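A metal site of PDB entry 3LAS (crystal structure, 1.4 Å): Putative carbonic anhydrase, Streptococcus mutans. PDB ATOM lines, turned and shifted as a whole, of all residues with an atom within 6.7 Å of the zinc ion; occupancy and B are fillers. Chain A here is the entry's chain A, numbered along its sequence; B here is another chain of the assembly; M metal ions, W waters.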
ATOM      1  N   CYS A  38      -9.062  -4.560  -9.125  1.00  0.00           N
ATOM      2  CA  CYS A  38      -9.073  -4.585 -10.568  1.00  0.00           C
ATOM      3  C   CYS A  38     -10.304  -3.899 -11.118  1.00  0.00           C
ATOM      4  O   CYS A  38     -11.391  -3.850 -10.487  1.00  0.00           O
ATOM      5  CB  CYS A  38      -9.051  -6.079 -10.982  1.00  0.00           C
ATOM      6  SG  CYS A  38      -8.903  -6.243 -12.842  1.00  0.00           S
ATOM      7  N   MET A  39     -10.164  -3.432 -12.354  1.00  0.00           N
ATOM      8  CA  MET A  39     -11.227  -2.860 -13.191  1.00  0.00           C
ATOM      9  C   MET A  39     -12.312  -3.800 -13.619  1.00  0.00           C
ATOM     10  O   MET A  39     -13.334  -3.381 -14.202  1.00  0.00           O
ATOM     11  CB  MET A  39     -10.611  -2.153 -14.396  1.00  0.00           C
ATOM     12  CG  MET A  39     -10.050  -3.266 -15.380  1.00  0.00           C
ATOM     13  SD  MET A  39      -9.043  -2.424 -16.680  1.00  0.00           S
ATOM     14  CE  MET A  39      -8.594  -3.854 -17.631  1.00  0.00           C
ATOM     15  N   ASP A  40     -12.108  -5.106 -13.377  1.00  0.00           N
ATOM     16  CA  ASP A  40     -12.988  -6.139 -13.866  1.00  0.00           C
ATOM     17  C   ASP A  40     -14.463  -5.811 -13.754  1.00  0.00           C
ATOM     18  O   ASP A  40     -14.977  -5.450 -12.702  1.00  0.00           O
ATOM     19  CB  ASP A  40     -12.704  -7.446 -13.123  1.00  0.00           C
ATOM     20  CG  ASP A  40     -13.344  -8.605 -13.832  1.00  0.00           C
ATOM     21  OD1 ASP A  40     -14.514  -8.949 -13.485  1.00  0.00           O
ATOM     22  OD2 ASP A  40     -12.651  -9.240 -14.633  1.00  0.00           O
ATOM     23  N   ARG A  42     -16.977  -7.628 -13.648  1.00  0.00           N
ATOM     24  CA  ARG A  42     -17.806  -8.550 -12.849  1.00  0.00           C
ATOM     25  C   ARG A  42     -17.631  -8.324 -11.370  1.00  0.00           C
ATOM     26  O   ARG A  42     -18.121  -9.124 -10.560  1.00  0.00           O
ATOM     27  CB  ARG A  42     -17.439  -9.982 -13.185  1.00  0.00           C
ATOM     28  CG  ARG A  42     -17.573 -10.280 -14.720  1.00  0.00           C
ATOM     29  CD  ARG A  42     -16.841 -11.541 -15.117  1.00  0.00           C
ATOM     30  NE  ARG A  42     -15.400 -11.343 -14.922  1.00  0.00           N
ATOM     31  CZ  ARG A  42     -14.508 -12.303 -15.135  1.00  0.00           C
ATOM     32  NH1 ARG A  42     -14.888 -13.521 -15.610  1.00  0.00           N
ATOM     33  NH2 ARG A  42     -13.246 -12.129 -14.792  1.00  0.00           N
ATOM     34  N   ASN A  61      -7.603  -0.548 -11.345  1.00  0.00           N
ATOM     35  CA  ASN A  61      -6.747  -0.555 -12.516  1.00  0.00           C
ATOM     36  C   ASN A  61      -6.712  -1.968 -13.077  1.00  0.00           C
ATOM     37  O   ASN A  61      -7.418  -2.872 -12.575  1.00  0.00           O
ATOM     38  CB  ASN A  61      -5.374   0.058 -12.279  1.00  0.00           C
ATOM     39  CG  ASN A  61      -4.519  -0.810 -11.342  1.00  0.00           C
ATOM     40  OD1 ASN A  61      -4.866  -1.974 -11.108  1.00  0.00           O
ATOM     41  ND2 ASN A  61      -3.391  -0.285 -10.939  1.00  0.00           N
ATOM     42  N   ALA A  62      -5.914  -2.203 -14.131  1.00  0.00           N
ATOM     43  CA  ALA A  62      -5.852  -3.591 -14.663  1.00  0.00           C
ATOM     44  C   ALA A  62      -5.032  -4.453 -13.689  1.00  0.00           C
ATOM     45  O   ALA A  62      -3.855  -4.215 -13.431  1.00  0.00           O
ATOM     46  CB  ALA A  62      -5.217  -3.624 -16.031  1.00  0.00           C
ATOM     47  N   GLY A  63      -5.726  -5.423 -13.097  1.00  0.00           N
ATOM     48  CA  GLY A  63      -5.132  -6.383 -12.166  1.00  0.00           C
ATOM     49  C   GLY A  63      -5.148  -5.937 -10.715  1.00  0.00           C
ATOM     50  O   GLY A  63      -4.854  -6.755  -9.823  1.00  0.00           O
ATOM     51  N   GLY A  64      -5.511  -4.699 -10.365  1.00  0.00           N
ATOM     52  CA  GLY A  64      -5.424  -4.248  -8.971  1.00  0.00           C
ATOM     53  C   GLY A  64      -3.957  -4.122  -8.586  1.00  0.00           C
ATOM     54  O   GLY A  64      -3.616  -4.380  -7.395  1.00  0.00           O
ATOM     55  N   HIS A  91      -8.583 -10.871  -7.871  1.00  0.00           N
ATOM     56  CA  HIS A  91      -9.769 -11.694  -8.117  1.00  0.00           C
ATOM     57  C   HIS A  91      -9.445 -12.800  -9.042  1.00  0.00           C
ATOM     58  O   HIS A  91      -8.420 -12.785  -9.752  1.00  0.00           O
ATOM     59  CB  HIS A  91     -10.921 -10.847  -8.661  1.00  0.00           C
ATOM     60  CG  HIS A  91     -10.725 -10.404 -10.088  1.00  0.00           C
ATOM     61  ND1 HIS A  91     -11.132 -11.140 -11.164  1.00  0.00           N
ATOM     62  CD2 HIS A  91     -10.025  -9.345 -10.607  1.00  0.00           C
ATOM     63  CE1 HIS A  91     -10.743 -10.539 -12.288  1.00  0.00           C
ATOM     64  NE2 HIS A  91     -10.040  -9.461 -11.956  1.00  0.00           N
ATOM     65  N   THR A  92     -10.325 -13.830  -9.047  1.00  0.00           N
ATOM     66  CA  THR A  92     -10.145 -15.026  -9.926  1.00  0.00           C
ATOM     67  C   THR A  92     -10.535 -14.675 -11.322  1.00  0.00           C
ATOM     68  O   THR A  92     -11.361 -13.764 -11.620  1.00  0.00           O
ATOM     69  CB  THR A  92     -11.020 -16.186  -9.372  1.00  0.00           C
ATOM     70  OG1 THR A  92     -12.414 -15.785  -9.438  1.00  0.00           O
ATOM     71  CG2 THR A  92     -10.591 -16.547  -7.925  1.00  0.00           C
ATOM     72  N   ASP A  93      -9.985 -15.414 -12.270  1.00  0.00           N
ATOM     73  CA  ASP A  93     -10.214 -15.220 -13.679  1.00  0.00           C
ATOM     74  C   ASP A  93      -9.861 -13.787 -14.091  1.00  0.00           C
ATOM     75  O   ASP A  93     -10.584 -13.143 -14.864  1.00  0.00           O
ATOM     76  CB  ASP A  93     -11.624 -15.594 -14.106  1.00  0.00           C
ATOM     77  CG  ASP A  93     -11.793 -15.722 -15.616  1.00  0.00           C
ATOM     78  OD1 ASP A  93     -10.826 -16.164 -16.312  1.00  0.00           O
ATOM     79  OD2 ASP A  93     -12.873 -15.427 -16.158  1.00  0.00           O
ATOM     80  N   CYS A  94      -8.743 -13.273 -13.649  1.00  0.00           N
ATOM     81  CA  CYS A  94      -8.312 -11.915 -13.981  1.00  0.00           C
ATOM     82  C   CYS A  94      -7.605 -11.890 -15.322  1.00  0.00           C
ATOM     83  O   CYS A  94      -6.834 -12.814 -15.711  1.00  0.00           O
ATOM     84  CB  CYS A  94      -7.395 -11.422 -12.913  1.00  0.00           C
ATOM     85  SG  CYS A  94      -6.826  -9.673 -13.116  1.00  0.00           S
ATOM     86  N   GLY A  95      -7.863 -10.822 -16.082  1.00  0.00           N
ATOM     87  CA  GLY A  95      -7.211 -10.599 -17.349  1.00  0.00           C
ATOM     88  C   GLY A  95      -5.705 -10.600 -17.217  1.00  0.00           C
ATOM     89  O   GLY A  95      -4.986 -10.969 -18.178  1.00  0.00           O
ATOM     90  N   ALA A  96      -5.154 -10.259 -16.031  1.00  0.00           N
ATOM     91  CA  ALA A  96      -3.682 -10.309 -15.861  1.00  0.00           C
ATOM     92  C   ALA A  96      -3.125 -11.649 -15.946  1.00  0.00           C
ATOM     93  O   ALA A  96      -1.858 -11.767 -16.123  1.00  0.00           O
ATOM     94  CB  ALA A  96      -3.366  -9.666 -14.441  1.00  0.00           C
ATOM     95  N   PHE A 124       0.274 -11.410 -13.991  1.00  0.00           N
ATOM     96  CA  PHE A 124       0.695 -12.328 -12.908  1.00  0.00           C
ATOM     97  C   PHE A 124       0.097 -13.687 -13.234  1.00  0.00           C
ATOM     98  O   PHE A 124      -0.937 -13.855 -13.981  1.00  0.00           O
ATOM     99  CB  PHE A 124       0.230 -11.788 -11.499  1.00  0.00           C
ATOM    100  CG  PHE A 124      -1.265 -11.652 -11.303  1.00  0.00           C
ATOM    101  CD1 PHE A 124      -2.062 -12.759 -11.106  1.00  0.00           C
ATOM    102  CD2 PHE A 124      -1.820 -10.403 -11.236  1.00  0.00           C
ATOM    103  CE1 PHE A 124      -3.446 -12.611 -10.850  1.00  0.00           C
ATOM    104  CE2 PHE A 124      -3.217 -10.237 -10.963  1.00  0.00           C
ATOM    105  CZ  PHE A 124      -3.984 -11.319 -10.805  1.00  0.00           C
ATOM    106  N   LEU B  27     -15.086 -12.486 -19.247  1.00  0.00           N
ATOM    107  CA  LEU B  27     -14.099 -11.455 -19.012  1.00  0.00           C
ATOM    108  C   LEU B  27     -14.334 -10.188 -19.815  1.00  0.00           C
ATOM    109  O   LEU B  27     -14.047  -9.063 -19.381  1.00  0.00           O
ATOM    110  CB  LEU B  27     -12.659 -12.002 -19.346  1.00  0.00           C
ATOM    111  CG  LEU B  27     -11.789 -12.120 -18.094  1.00  0.00           C
ATOM    112  CD1 LEU B  27     -10.521 -12.894 -18.398  1.00  0.00           C
ATOM    113  CD2 LEU B  27     -11.423 -10.829 -17.360  1.00  0.00           C
ATOM    114  N   LEU B  81      -8.963  -7.430 -23.861  1.00  0.00           N
ATOM    115  CA  LEU B  81     -10.306  -7.804 -23.321  1.00  0.00           C
ATOM    116  C   LEU B  81     -11.394  -7.208 -24.074  1.00  0.00           C
ATOM    117  O   LEU B  81     -12.528  -7.245 -23.607  1.00  0.00           O
ATOM    118  CB  LEU B  81     -10.341  -7.455 -21.782  1.00  0.00           C
ATOM    119  CG  LEU B  81      -9.224  -8.089 -20.920  1.00  0.00           C
ATOM    120  CD1 LEU B  81      -9.374  -7.573 -19.459  1.00  0.00           C
ATOM    121  CD2 LEU B  81      -9.290  -9.628 -20.900  1.00  0.00           C
HETATM  122 ZN    ZN M   1      -8.791  -8.483 -13.243  1.00  0.00          ZN
HETATM  123  O   HOH W   1      -9.711  -8.702 -15.184  1.00  0.00           O
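The side-chain sulfur (SG) of Cys 38 lies close to the backbone NH (N) of Asp 40 (3.4 Å).
The side-chain sulfur (SG) of Cys 94 sits close to the backbone NH (N) of Ala 96 (3.4 Å).
SG of Cys 38 lies close to O of Asn 61, at 3.7 Å.
The side-chain sulfur (SG) of Cys 38 sits close to the backbone NH (N) of Gly 63 (3.3 Å).
N of Gly 95 touches the zinc ion, 3.8 Å away.
Within 4 Å of the zinc ion: Cys 38, His 91, Cys 94 and Gly 95.
The nearest printed residue that does not touch the zinc ion is Asp 40 (4.05 Å).
The zinc ion is bound by a ring nitrogen (NE2) of His 91 (2.0 Å), water W1 (2.2 Å), the side-chain sulfur (SG) of Cys 38 (2.3 Å) and the side-chain sulfur (SG) of Cys 94 (2.3 Å).
The zinc ion has four donor atoms within binding distance.
Water W1 bridges the backbone NH of Gly 95 (3.0 Å) and the side-chain carboxylate of Asp 40 (3.0 Å).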
